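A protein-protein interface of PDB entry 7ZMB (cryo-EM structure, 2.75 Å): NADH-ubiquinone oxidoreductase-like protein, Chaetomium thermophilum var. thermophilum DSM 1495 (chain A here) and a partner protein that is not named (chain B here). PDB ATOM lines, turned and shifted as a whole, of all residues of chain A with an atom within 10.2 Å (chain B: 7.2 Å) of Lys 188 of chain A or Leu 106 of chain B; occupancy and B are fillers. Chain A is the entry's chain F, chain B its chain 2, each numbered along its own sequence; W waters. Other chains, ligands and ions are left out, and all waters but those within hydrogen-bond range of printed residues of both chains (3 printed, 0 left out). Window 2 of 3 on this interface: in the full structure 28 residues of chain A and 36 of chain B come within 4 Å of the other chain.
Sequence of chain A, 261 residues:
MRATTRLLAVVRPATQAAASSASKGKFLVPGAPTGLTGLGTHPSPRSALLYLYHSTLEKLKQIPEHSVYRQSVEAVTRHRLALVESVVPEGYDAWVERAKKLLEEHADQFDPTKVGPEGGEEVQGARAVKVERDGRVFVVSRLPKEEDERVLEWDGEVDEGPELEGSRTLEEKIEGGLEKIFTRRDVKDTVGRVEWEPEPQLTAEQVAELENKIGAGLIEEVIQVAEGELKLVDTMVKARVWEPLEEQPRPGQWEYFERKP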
ATOM      1  N   GLU A 122     -13.205 -24.905   7.858  1.00  0.00           N
ATOM      2  CA  GLU A 122     -14.590 -24.467   7.730  1.00  0.00           C
ATOM      3  C   GLU A 122     -15.239 -24.489   9.110  1.00  0.00           C
ATOM      4  O   GLU A 122     -15.679 -25.536   9.585  1.00  0.00           O
ATOM      5  CB  GLU A 122     -15.335 -25.353   6.739  1.00  0.00           C
ATOM      6  CG  GLU A 122     -14.852 -25.233   5.289  1.00  0.00           C
ATOM      7  CD  GLU A 122     -13.623 -26.082   4.995  1.00  0.00           C
ATOM      8  OE1 GLU A 122     -13.178 -26.817   5.902  1.00  0.00           O
ATOM      9  OE2 GLU A 122     -13.100 -26.018   3.862  1.00  0.00           O
ATOM     10  N   GLN A 124     -18.066 -23.170   9.940  1.00  0.00           N
ATOM     11  CA  GLN A 124     -19.518 -23.202   9.854  1.00  0.00           C
ATOM     12  C   GLN A 124     -20.076 -24.612   9.687  1.00  0.00           C
ATOM     13  O   GLN A 124     -21.299 -24.780   9.645  1.00  0.00           O
ATOM     14  CB  GLN A 124     -19.974 -22.302   8.704  1.00  0.00           C
ATOM     15  CG  GLN A 124     -19.671 -22.877   7.356  1.00  0.00           C
ATOM     16  CD  GLN A 124     -18.316 -22.454   6.854  1.00  0.00           C
ATOM     17  OE1 GLN A 124     -17.292 -22.861   7.394  1.00  0.00           O
ATOM     18  NE2 GLN A 124     -18.299 -21.675   5.789  1.00  0.00           N
ATOM     19  N   GLY A 125     -19.214 -25.623   9.575  1.00  0.00           N
ATOM     20  CA  GLY A 125     -19.608 -27.005   9.709  1.00  0.00           C
ATOM     21  C   GLY A 125     -18.935 -27.651  10.910  1.00  0.00           C
ATOM     22  O   GLY A 125     -18.165 -27.023  11.634  1.00  0.00           O
ATOM     23  N   ALA A 126     -19.250 -28.926  11.103  1.00  0.00           N
ATOM     24  CA  ALA A 126     -18.645 -29.702  12.175  1.00  0.00           C
ATOM     25  C   ALA A 126     -17.198 -30.050  11.848  1.00  0.00           C
ATOM     26  O   ALA A 126     -16.827 -30.248  10.688  1.00  0.00           O
ATOM     27  CB  ALA A 126     -19.441 -30.978  12.422  1.00  0.00           C
ATOM     28  N   TRP A 154     -24.393 -16.140   5.432  1.00  0.00           N
ATOM     29  CA  TRP A 154     -23.696 -17.233   4.702  1.00  0.00           C
ATOM     30  C   TRP A 154     -23.498 -18.471   5.581  1.00  0.00           C
ATOM     31  O   TRP A 154     -22.417 -19.061   5.489  1.00  0.00           O
ATOM     32  CB  TRP A 154     -22.389 -16.733   4.090  1.00  0.00           C
ATOM     33  CG  TRP A 154     -22.584 -15.606   3.124  1.00  0.00           C
ATOM     34  CD1 TRP A 154     -23.169 -15.675   1.895  1.00  0.00           C
ATOM     35  CD2 TRP A 154     -22.200 -14.231   3.306  1.00  0.00           C
ATOM     36  NE1 TRP A 154     -23.164 -14.447   1.294  1.00  0.00           N
ATOM     37  CE2 TRP A 154     -22.575 -13.541   2.134  1.00  0.00           C
ATOM     38  CE3 TRP A 154     -21.568 -13.522   4.332  1.00  0.00           C
ATOM     39  CZ2 TRP A 154     -22.348 -12.176   1.970  1.00  0.00           C
ATOM     40  CZ3 TRP A 154     -21.342 -12.174   4.169  1.00  0.00           C
ATOM     41  CH2 TRP A 154     -21.732 -11.514   3.005  1.00  0.00           C
ATOM     42  N   ASP A 155     -24.477 -18.807   6.425  1.00  0.00           N
ATOM     43  CA  ASP A 155     -24.415 -20.018   7.284  1.00  0.00           C
ATOM     44  C   ASP A 155     -23.359 -19.847   8.371  1.00  0.00           C
ATOM     45  O   ASP A 155     -23.079 -20.837   9.064  1.00  0.00           O
ATOM     46  CB  ASP A 155     -24.184 -21.296   6.473  1.00  0.00           C
ATOM     47  CG  ASP A 155     -25.282 -21.575   5.463  1.00  0.00           C
ATOM     48  OD1 ASP A 155     -26.450 -21.284   5.777  1.00  0.00           O
ATOM     49  OD2 ASP A 155     -24.956 -22.069   4.368  1.00  0.00           O
ATOM     50  N   GLU A 157     -20.254 -18.556   7.524  1.00  0.00           N
ATOM     51  CA  GLU A 157     -18.938 -18.624   6.834  1.00  0.00           C
ATOM     52  C   GLU A 157     -17.993 -17.556   7.393  1.00  0.00           C
ATOM     53  O   GLU A 157     -18.482 -16.523   7.851  1.00  0.00           O
ATOM     54  CB  GLU A 157     -19.150 -18.555   5.323  1.00  0.00           C
ATOM     55  CG  GLU A 157     -17.900 -18.814   4.505  1.00  0.00           C
ATOM     56  CD  GLU A 157     -18.173 -19.381   3.126  1.00  0.00           C
ATOM     57  OE1 GLU A 157     -19.329 -19.291   2.668  1.00  0.00           O
ATOM     58  OE2 GLU A 157     -17.233 -19.933   2.524  1.00  0.00           O
ATOM     59  N   ILE A 181      -8.726 -22.458  -2.953  1.00  0.00           N
ATOM     60  CA  ILE A 181      -9.743 -22.977  -3.863  1.00  0.00           C
ATOM     61  C   ILE A 181      -9.640 -24.488  -3.985  1.00  0.00           C
ATOM     62  O   ILE A 181     -10.652 -25.189  -4.099  1.00  0.00           O
ATOM     63  CB  ILE A 181      -9.656 -22.280  -5.239  1.00  0.00           C
ATOM     64  CG1 ILE A 181      -9.903 -20.774  -5.100  1.00  0.00           C
ATOM     65  CG2 ILE A 181     -10.583 -22.925  -6.264  1.00  0.00           C
ATOM     66  CD1 ILE A 181      -8.696 -19.939  -4.937  1.00  0.00           C
ATOM     67  N   ARG A 184     -10.134 -26.158   0.216  1.00  0.00           N
ATOM     68  CA  ARG A 184     -11.315 -25.898   1.016  1.00  0.00           C
ATOM     69  C   ARG A 184     -12.513 -26.663   0.464  1.00  0.00           C
ATOM     70  O   ARG A 184     -12.535 -27.098  -0.690  1.00  0.00           O
ATOM     71  CB  ARG A 184     -11.596 -24.397   1.070  1.00  0.00           C
ATOM     72  CG  ARG A 184     -10.991 -23.744   2.283  1.00  0.00           C
ATOM     73  CD  ARG A 184     -11.291 -22.286   2.368  1.00  0.00           C
ATOM     74  NE  ARG A 184     -10.203 -21.590   3.032  1.00  0.00           N
ATOM     75  CZ  ARG A 184     -10.067 -20.272   3.058  1.00  0.00           C
ATOM     76  NH1 ARG A 184     -10.960 -19.502   2.456  1.00  0.00           N
ATOM     77  NH2 ARG A 184      -9.042 -19.721   3.692  1.00  0.00           N
ATOM     78  N   ARG A 185     -13.511 -26.843   1.313  1.00  0.00           N
ATOM     79  CA  ARG A 185     -14.655 -27.676   0.992  1.00  0.00           C
ATOM     80  C   ARG A 185     -15.953 -26.896   1.106  1.00  0.00           C
ATOM     81  O   ARG A 185     -16.146 -26.122   2.044  1.00  0.00           O
ATOM     82  CB  ARG A 185     -14.722 -28.893   1.903  1.00  0.00           C
ATOM     83  CG  ARG A 185     -15.466 -30.056   1.292  1.00  0.00           C
ATOM     84  CD  ARG A 185     -15.729 -31.139   2.316  1.00  0.00           C
ATOM     85  NE  ARG A 185     -16.527 -30.669   3.448  1.00  0.00           N
ATOM     86  CZ  ARG A 185     -16.062 -30.562   4.687  1.00  0.00           C
ATOM     87  NH1 ARG A 185     -14.806 -30.878   4.950  1.00  0.00           N
ATOM     88  NH2 ARG A 185     -16.851 -30.137   5.661  1.00  0.00           N
ATOM     89  N   ASP A 186     -16.831 -27.097   0.132  1.00  0.00           N
ATOM     90  CA  ASP A 186     -18.219 -26.713   0.302  1.00  0.00           C
ATOM     91  C   ASP A 186     -18.808 -27.564   1.410  1.00  0.00           C
ATOM     92  O   ASP A 186     -18.706 -28.792   1.372  1.00  0.00           O
ATOM     93  CB  ASP A 186     -18.983 -26.903  -1.008  1.00  0.00           C
ATOM     94  CG  ASP A 186     -20.432 -26.470  -0.911  1.00  0.00           C
ATOM     95  OD1 ASP A 186     -20.696 -25.252  -0.880  1.00  0.00           O
ATOM     96  OD2 ASP A 186     -21.308 -27.354  -0.862  1.00  0.00           O
ATOM     97  N   VAL A 187     -19.400 -26.913   2.411  1.00  0.00           N
ATOM     98  CA  VAL A 187     -19.824 -27.628   3.610  1.00  0.00           C
ATOM     99  C   VAL A 187     -20.879 -28.666   3.262  1.00  0.00           C
ATOM    100  O   VAL A 187     -20.916 -29.756   3.844  1.00  0.00           O
ATOM    101  CB  VAL A 187     -20.330 -26.635   4.673  1.00  0.00           C
ATOM    102  CG1 VAL A 187     -20.777 -27.366   5.926  1.00  0.00           C
ATOM    103  CG2 VAL A 187     -19.249 -25.619   5.007  1.00  0.00           C
ATOM    104  N   LYS A 188     -21.744 -28.353   2.297  1.00  0.00           N
ATOM    105  CA  LYS A 188     -22.761 -29.300   1.867  1.00  0.00           C
ATOM    106  C   LYS A 188     -22.173 -30.502   1.140  1.00  0.00           C
ATOM    107  O   LYS A 188     -22.881 -31.495   0.950  1.00  0.00           O
ATOM    108  CB  LYS A 188     -23.781 -28.591   0.976  1.00  0.00           C
ATOM    109  CG  LYS A 188     -24.515 -27.459   1.668  1.00  0.00           C
ATOM    110  CD  LYS A 188     -25.339 -26.646   0.683  1.00  0.00           C
ATOM    111  CE  LYS A 188     -24.447 -25.879  -0.283  1.00  0.00           C
ATOM    112  NZ  LYS A 188     -23.578 -24.895   0.414  1.00  0.00           N
ATOM    113  N   ASP A 189     -20.911 -30.439   0.726  1.00  0.00           N
ATOM    114  CA  ASP A 189     -20.244 -31.580   0.101  1.00  0.00           C
ATOM    115  C   ASP A 189     -19.808 -32.558   1.182  1.00  0.00           C
ATOM    116  O   ASP A 189     -18.745 -32.418   1.785  1.00  0.00           O
ATOM    117  CB  ASP A 189     -19.053 -31.127  -0.728  1.00  0.00           C
ATOM    118  CG  ASP A 189     -18.217 -32.293  -1.220  1.00  0.00           C
ATOM    119  OD1 ASP A 189     -18.808 -33.344  -1.548  1.00  0.00           O
ATOM    120  OD2 ASP A 189     -16.977 -32.164  -1.272  1.00  0.00           O
ATOM    121  N   THR A 190     -20.638 -33.571   1.432  1.00  0.00           N
ATOM    122  CA  THR A 190     -20.354 -34.600   2.438  1.00  0.00           C
ATOM    123  C   THR A 190     -20.655 -35.970   1.835  1.00  0.00           C
ATOM    124  O   THR A 190     -21.769 -36.484   1.966  1.00  0.00           O
ATOM    125  CB  THR A 190     -21.167 -34.364   3.711  1.00  0.00           C
ATOM    126  OG1 THR A 190     -22.564 -34.397   3.395  1.00  0.00           O
ATOM    127  CG2 THR A 190     -20.822 -33.021   4.337  1.00  0.00           C
ATOM    128  N   VAL A 191     -19.660 -36.567   1.177  1.00  0.00           N
ATOM    129  CA  VAL A 191     -19.746 -37.943   0.711  1.00  0.00           C
ATOM    130  C   VAL A 191     -18.578 -38.787   1.202  1.00  0.00           C
ATOM    131  O   VAL A 191     -18.775 -39.919   1.657  1.00  0.00           O
ATOM    132  CB  VAL A 191     -19.867 -38.016  -0.828  1.00  0.00           C
ATOM    133  CG1 VAL A 191     -21.258 -37.586  -1.257  1.00  0.00           C
ATOM    134  CG2 VAL A 191     -18.824 -37.150  -1.496  1.00  0.00           C
ATOM    135  N   GLY A 192     -17.359 -38.264   1.128  1.00  0.00           N
ATOM    136  CA  GLY A 192     -16.185 -38.971   1.591  1.00  0.00           C
ATOM    137  C   GLY A 192     -15.911 -38.851   3.073  1.00  0.00           C
ATOM    138  O   GLY A 192     -14.822 -39.215   3.525  1.00  0.00           O
ATOM    139  N   ARG A 193     -16.869 -38.348   3.845  1.00  0.00           N
ATOM    140  CA  ARG A 193     -16.678 -38.051   5.254  1.00  0.00           C
ATOM    141  C   ARG A 193     -17.799 -38.681   6.065  1.00  0.00           C
ATOM    142  O   ARG A 193     -18.884 -38.957   5.550  1.00  0.00           O
ATOM    143  CB  ARG A 193     -16.647 -36.542   5.490  1.00  0.00           C
ATOM    144  CG  ARG A 193     -15.514 -35.851   4.787  1.00  0.00           C
ATOM    145  CD  ARG A 193     -15.688 -34.353   4.812  1.00  0.00           C
ATOM    146  NE  ARG A 193     -15.673 -33.821   6.165  1.00  0.00           N
ATOM    147  CZ  ARG A 193     -14.566 -33.524   6.825  1.00  0.00           C
ATOM    148  NH1 ARG A 193     -14.635 -33.027   8.050  1.00  0.00           N
ATOM    149  NH2 ARG A 193     -13.387 -33.739   6.263  1.00  0.00           N
ATOM    150  N   LYS B 104     -27.683 -30.654  -9.289  1.00  0.00           N
ATOM    151  CA  LYS B 104     -27.009 -29.653  -8.484  1.00  0.00           C
ATOM    152  C   LYS B 104     -25.514 -29.871  -8.603  1.00  0.00           C
ATOM    153  O   LYS B 104     -25.057 -30.994  -8.816  1.00  0.00           O
ATOM    154  CB  LYS B 104     -27.424 -29.741  -7.024  1.00  0.00           C
ATOM    155  CG  LYS B 104     -28.910 -29.715  -6.809  1.00  0.00           C
ATOM    156  CD  LYS B 104     -29.249 -29.581  -5.334  1.00  0.00           C
ATOM    157  CE  LYS B 104     -30.752 -29.519  -5.120  1.00  0.00           C
ATOM    158  NZ  LYS B 104     -31.424 -30.783  -5.526  1.00  0.00           N
ATOM    159  N   ILE B 105     -24.748 -28.797  -8.470  1.00  0.00           N
ATOM    160  CA  ILE B 105     -23.295 -28.887  -8.503  1.00  0.00           C
ATOM    161  C   ILE B 105     -22.740 -28.289  -7.223  1.00  0.00           C
ATOM    162  O   ILE B 105     -22.872 -27.084  -6.985  1.00  0.00           O
ATOM    163  CB  ILE B 105     -22.700 -28.212  -9.748  1.00  0.00           C
ATOM    164  CG1 ILE B 105     -23.280 -26.818  -9.964  1.00  0.00           C
ATOM    165  CG2 ILE B 105     -22.942 -29.086 -10.960  1.00  0.00           C
ATOM    166  CD1 ILE B 105     -22.386 -25.911 -10.762  1.00  0.00           C
ATOM    167  N   LEU B 106     -22.112 -29.128  -6.408  1.00  0.00           N
ATOM    168  CA  LEU B 106     -21.466 -28.700  -5.175  1.00  0.00           C
ATOM    169  C   LEU B 106     -19.982 -28.476  -5.411  1.00  0.00           C
ATOM    170  O   LEU B 106     -19.299 -29.344  -5.954  1.00  0.00           O
ATOM    171  CB  LEU B 106     -21.649 -29.736  -4.069  1.00  0.00           C
ATOM    172  CG  LEU B 106     -23.022 -29.914  -3.436  1.00  0.00           C
ATOM    173  CD1 LEU B 106     -22.930 -30.973  -2.371  1.00  0.00           C
ATOM    174  CD2 LEU B 106     -23.521 -28.613  -2.859  1.00  0.00           C
ATOM    175  N   TYR B 107     -19.489 -27.319  -4.985  1.00  0.00           N
ATOM    176  CA  TYR B 107     -18.064 -27.019  -4.991  1.00  0.00           C
ATOM    177  C   TYR B 107     -17.841 -25.769  -4.160  1.00  0.00           C
ATOM    178  O   TYR B 107     -18.779 -25.029  -3.863  1.00  0.00           O
ATOM    179  CB  TYR B 107     -17.527 -26.843  -6.416  1.00  0.00           C
ATOM    180  CG  TYR B 107     -17.995 -25.596  -7.135  1.00  0.00           C
ATOM    181  CD1 TYR B 107     -19.283 -25.500  -7.646  1.00  0.00           C
ATOM    182  CD2 TYR B 107     -17.144 -24.517  -7.306  1.00  0.00           C
ATOM    183  CE1 TYR B 107     -19.697 -24.371  -8.300  1.00  0.00           C
ATOM    184  CE2 TYR B 107     -17.553 -23.389  -7.953  1.00  0.00           C
ATOM    185  CZ  TYR B 107     -18.826 -23.316  -8.450  1.00  0.00           C
ATOM    186  OH  TYR B 107     -19.220 -22.175  -9.101  1.00  0.00           O
ATOM    187  N   TYR B 108     -16.590 -25.537  -3.785  1.00  0.00           N
ATOM    188  CA  TYR B 108     -16.231 -24.328  -3.048  1.00  0.00           C
ATOM    189  C   TYR B 108     -16.274 -23.147  -4.010  1.00  0.00           C
ATOM    190  O   TYR B 108     -15.349 -22.939  -4.798  1.00  0.00           O
ATOM    191  CB  TYR B 108     -14.853 -24.469  -2.413  1.00  0.00           C
ATOM    192  CG  TYR B 108     -14.525 -23.332  -1.478  1.00  0.00           C
ATOM    193  CD1 TYR B 108     -15.461 -22.874  -0.563  1.00  0.00           C
ATOM    194  CD2 TYR B 108     -13.312 -22.671  -1.552  1.00  0.00           C
ATOM    195  CE1 TYR B 108     -15.181 -21.824   0.277  1.00  0.00           C
ATOM    196  CE2 TYR B 108     -13.030 -21.606  -0.721  1.00  0.00           C
ATOM    197  CZ  TYR B 108     -13.970 -21.187   0.187  1.00  0.00           C
ATOM    198  OH  TYR B 108     -13.694 -20.138   1.028  1.00  0.00           O
ATOM    199  N   ARG B 109     -17.295 -22.305  -3.894  1.00  0.00           N
ATOM    200  CA  ARG B 109     -17.425 -21.175  -4.850  1.00  0.00           C
ATOM    201  C   ARG B 109     -17.104 -19.846  -4.171  1.00  0.00           C
ATOM    202  O   ARG B 109     -17.105 -18.847  -4.884  1.00  0.00           O
ATOM    203  CB  ARG B 109     -18.852 -21.043  -5.380  1.00  0.00           C
ATOM    204  CG  ARG B 109     -19.781 -22.219  -5.146  1.00  0.00           C
ATOM    205  CD  ARG B 109     -21.055 -21.945  -5.924  1.00  0.00           C
ATOM    206  NE  ARG B 109     -21.871 -23.128  -6.142  1.00  0.00           N
ATOM    207  CZ  ARG B 109     -22.858 -23.214  -7.025  1.00  0.00           C
ATOM    208  NH1 ARG B 109     -23.153 -22.181  -7.793  1.00  0.00           N
ATOM    209  NH2 ARG B 109     -23.537 -24.338  -7.147  1.00  0.00           N
ATOM    210  N   LYS B 115     -18.221 -14.227  -3.600  1.00  0.00           N
ATOM    211  CA  LYS B 115     -19.509 -14.178  -2.864  1.00  0.00           C
ATOM    212  C   LYS B 115     -19.524 -13.006  -1.889  1.00  0.00           C
ATOM    213  O   LYS B 115     -20.579 -12.357  -1.773  1.00  0.00           O
ATOM    214  CB  LYS B 115     -19.699 -15.499  -2.113  1.00  0.00           C
ATOM    215  CG  LYS B 115     -20.959 -15.641  -1.276  1.00  0.00           C
ATOM    216  CD  LYS B 115     -20.942 -16.916  -0.466  1.00  0.00           C
ATOM    217  CE  LYS B 115     -20.459 -18.106  -1.266  1.00  0.00           C
ATOM    218  NZ  LYS B 115     -20.579 -19.372  -0.507  1.00  0.00           N
ATOM    219  N   PHE B 508      -9.768 -28.156  -7.787  1.00  0.00           N
ATOM    220  CA  PHE B 508     -10.851 -28.305  -6.830  1.00  0.00           C
ATOM    221  C   PHE B 508     -11.824 -29.377  -7.293  1.00  0.00           C
ATOM    222  O   PHE B 508     -11.918 -29.696  -8.478  1.00  0.00           O
ATOM    223  CB  PHE B 508     -11.580 -26.977  -6.596  1.00  0.00           C
ATOM    224  CG  PHE B 508     -12.186 -26.364  -7.830  1.00  0.00           C
ATOM    225  CD1 PHE B 508     -11.410 -25.639  -8.717  1.00  0.00           C
ATOM    226  CD2 PHE B 508     -13.542 -26.481  -8.082  1.00  0.00           C
ATOM    227  CE1 PHE B 508     -11.968 -25.061  -9.832  1.00  0.00           C
ATOM    228  CE2 PHE B 508     -14.107 -25.907  -9.206  1.00  0.00           C
ATOM    229  CZ  PHE B 508     -13.317 -25.190 -10.079  1.00  0.00           C
ATOM    230  N   SER B 509     -12.541 -29.942  -6.336  1.00  0.00           N
ATOM    231  CA  SER B 509     -13.476 -31.021  -6.605  1.00  0.00           C
ATOM    232  C   SER B 509     -14.883 -30.458  -6.761  1.00  0.00           C
ATOM    233  O   SER B 509     -15.402 -29.809  -5.848  1.00  0.00           O
ATOM    234  CB  SER B 509     -13.441 -32.056  -5.485  1.00  0.00           C
ATOM    235  OG  SER B 509     -14.456 -33.022  -5.669  1.00  0.00           O
ATOM    236  N   LEU B 510     -15.496 -30.715  -7.909  1.00  0.00           N
ATOM    237  CA  LEU B 510     -16.912 -30.464  -8.100  1.00  0.00           C
ATOM    238  C   LEU B 510     -17.638 -31.796  -8.142  1.00  0.00           C
ATOM    239  O   LEU B 510     -17.097 -32.814  -8.576  1.00  0.00           O
ATOM    240  CB  LEU B 510     -17.172 -29.651  -9.374  1.00  0.00           C
ATOM    241  CG  LEU B 510     -18.580 -29.124  -9.665  1.00  0.00           C
ATOM    242  CD1 LEU B 510     -18.506 -27.857 -10.495  1.00  0.00           C
ATOM    243  CD2 LEU B 510     -19.418 -30.148 -10.395  1.00  0.00           C
ATOM    244  N   ARG B 511     -18.868 -31.784  -7.646  1.00  0.00           N
ATOM    245  CA  ARG B 511     -19.635 -33.001  -7.471  1.00  0.00           C
ATOM    246  C   ARG B 511     -21.052 -32.718  -7.936  1.00  0.00           C
ATOM    247  O   ARG B 511     -21.632 -31.695  -7.569  1.00  0.00           O
ATOM    248  CB  ARG B 511     -19.568 -33.436  -6.005  1.00  0.00           C
ATOM    249  CG  ARG B 511     -18.148 -33.857  -5.658  1.00  0.00           C
ATOM    250  CD  ARG B 511     -17.889 -34.304  -4.256  1.00  0.00           C
ATOM    251  NE  ARG B 511     -16.475 -34.635  -4.135  1.00  0.00           N
ATOM    252  CZ  ARG B 511     -15.866 -35.007  -3.014  1.00  0.00           C
ATOM    253  NH1 ARG B 511     -14.572 -35.292  -3.029  1.00  0.00           N
ATOM    254  NH2 ARG B 511     -16.532 -35.056  -1.871  1.00  0.00           N
ATOM    255  N   ILE B 512     -21.590 -33.604  -8.766  1.00  0.00           N
ATOM    256  CA  ILE B 512     -22.884 -33.408  -9.404  1.00  0.00           C
ATOM    257  C   ILE B 512     -23.882 -34.347  -8.751  1.00  0.00           C
ATOM    258  O   ILE B 512     -23.706 -35.568  -8.784  1.00  0.00           O
ATOM    259  CB  ILE B 512     -22.818 -33.648 -10.920  1.00  0.00           C
ATOM    260  CG1 ILE B 512     -21.644 -32.892 -11.533  1.00  0.00           C
ATOM    261  CG2 ILE B 512     -24.126 -33.241 -11.589  1.00  0.00           C
ATOM    262  CD1 ILE B 512     -21.550 -33.058 -13.009  1.00  0.00           C
ATOM    263  N   LEU B 513     -24.924 -33.779  -8.163  1.00  0.00           N
ATOM    264  CA  LEU B 513     -25.998 -34.533  -7.539  1.00  0.00           C
ATOM    265  C   LEU B 513     -27.258 -34.419  -8.384  1.00  0.00           C
ATOM    266  O   LEU B 513     -27.359 -33.587  -9.285  1.00  0.00           O
ATOM    267  CB  LEU B 513     -26.263 -34.038  -6.112  1.00  0.00           C
ATOM    268  CG  LEU B 513     -25.314 -34.451  -4.986  1.00  0.00           C
ATOM    269  CD1 LEU B 513     -23.968 -33.755  -5.086  1.00  0.00           C
ATOM    270  CD2 LEU B 513     -25.949 -34.199  -3.632  1.00  0.00           C
ATOM    271  N   ASN B 517     -30.635 -35.143  -3.634  1.00  0.00           N
ATOM    272  CA  ASN B 517     -29.448 -35.257  -2.785  1.00  0.00           C
ATOM    273  C   ASN B 517     -28.764 -36.615  -2.902  1.00  0.00           C
ATOM    274  O   ASN B 517     -28.430 -37.261  -1.907  1.00  0.00           O
ATOM    275  CB  ASN B 517     -29.807 -34.960  -1.331  1.00  0.00           C
ATOM    276  CG  ASN B 517     -30.372 -33.570  -1.147  1.00  0.00           C
ATOM    277  OD1 ASN B 517     -29.784 -32.585  -1.589  1.00  0.00           O
ATOM    278  ND2 ASN B 517     -31.528 -33.484  -0.500  1.00  0.00           N
ATOM    279  N   VAL B 523     -16.123 -34.518 -10.116  1.00  0.00           N
ATOM    280  CA  VAL B 523     -15.245 -33.970 -11.136  1.00  0.00           C
ATOM    281  C   VAL B 523     -14.114 -33.223 -10.443  1.00  0.00           C
ATOM    282  O   VAL B 523     -14.268 -32.725  -9.324  1.00  0.00           O
ATOM    283  CB  VAL B 523     -16.021 -33.040 -12.098  1.00  0.00           C
ATOM    284  CG1 VAL B 523     -15.119 -32.504 -13.178  1.00  0.00           C
ATOM    285  CG2 VAL B 523     -17.211 -33.768 -12.708  1.00  0.00           C
HETATM  286  O   HOH W   1     -18.820 -22.482  -1.388  1.00  0.00           O
HETATM  287  O   HOH W   2     -21.326 -24.990  -4.159  1.00  0.00           O
HETATM  288  O   HOH W   3     -23.928 -12.689  -1.495  1.00  0.00           O
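Among the printed residues, merely in contact across the chains: Val 191 of chain A with Arg 511 of chain B (3.1 Å), Ile 181 of chain A with Phe 508 of chain B (3.2 Å), Asp 186 of chain A with Leu 106 of chain B (3.2 Å), Lys 188 of chain A with Leu 106 of chain B (3.4 Å), Asp 186 of chain A with Tyr 107 of chain B (3.4 Å), Trp 154 of chain A with Lys 115 of chain B (3.5 Å), Glu 157 of chain A with Tyr 108 of chain B (3.6 Å), Asp 189 of chain A with Leu 106 of chain B (3.7 Å) and Asp 186 of chain A with Tyr 108 of chain B (3.9 Å).
NH1 of Arg 184 of chain A sits at hydrogen-bond distance from OH of Tyr 108 of chain B (3.1 Å).
NZ of Lys 115 of chain B is in salt-bridge range of OE1 of Glu 157 of chain A, at 3.4 Å.
The guanidinium group of Arg 511 of chain B is in salt-bridge range of the side-chain carboxylate of Asp 189 of chain A (2.9 Å).
Printed residues of chain B within 4 Å of Glu 157 of chain A: Tyr 108 (3.6 Å) and Lys 115 (3.4 Å).
Printed residues of chain B within 4 Å of Asp 186 of chain A: Leu 106 (3.2 Å), Tyr 107 (3.4 Å) and Tyr 108 (3.9 Å).
Lys 188 of chain A touches just one residue of chain B: Leu 106 (3.4 Å).
No residue of chain A comes within 4 Å of Ile 105 of chain B.
Of chain A, only Asp 186 (3.2 Å), Lys 188 (3.4 Å) and Asp 189 (3.7 Å) come within 4 Å of Leu 106 of chain B.
Printed residues of chain A within 4 Å of Phe 508 of chain B: Ile 181.
No residue of chain A comes within 4 Å of Leu 510 of chain B.
The nearest residue of chain B that does not touch Lys 188 of chain A is Leu 513 of chain B (6.1 Å).
The nearest residue of chain A that does not touch Leu 106 of chain B is Thr 190 of chain A (5.1 Å).
The nearest printed residue of chain B that does not touch Val 191 of chain A is Leu 513 of chain B (6.1 Å).
Water W2 lies within hydrogen-bond range of the backbone carbonyl oxygen of Tyr 107 of chain B, the guanidinium group of Arg 109 of chain B and the side-chain carboxylate of Asp 186 of chain A.
Water W1 bridges N of Arg 109 of chain B and OD1 of Asp 186 of chain A.
Water W3 bridges the backbone carbonyl oxygen (O) of Lys 115 of chain B and the indole nitrogen (NE1) of Trp 154 of chain A.
The guanidinium group (NE) of Arg 185 of chain A is in hydrogen-bond range of the backbone carbonyl oxygen (O) of Asp 189 of chain A (3.3 Å).
The backbone NH of Leu 106 of chain B sits at hydrogen-bond distance from the backbone carbonyl oxygen of Arg 511 of chain B (2.9 Å).
OG of Ser 509 of chain B lies within hydrogen-bond range of NE of Arg 511 of chain B (3.0 Å).
N of Asp 189 of chain A lies within hydrogen-bond range of OD2 of Asp 186 of chain A (3.5 Å).
The side-chain carboxylate (OD1) of Asp 186 of chain A lies within salt-bridge range of the side-chain amino group (NZ) of Lys 188 of chain A.
Among the printed residues, 12 pairs touch across the chains.
Among the printed residues, Asp or Glu carboxylates within 4 Å of a Lys or Arg side-chain nitrogen of the other chain: Glu 157 of chain A with Lys 115 of chain B (3.4 Å) and Asp 189 of chain A with Arg 511 of chain B (2.9 Å).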
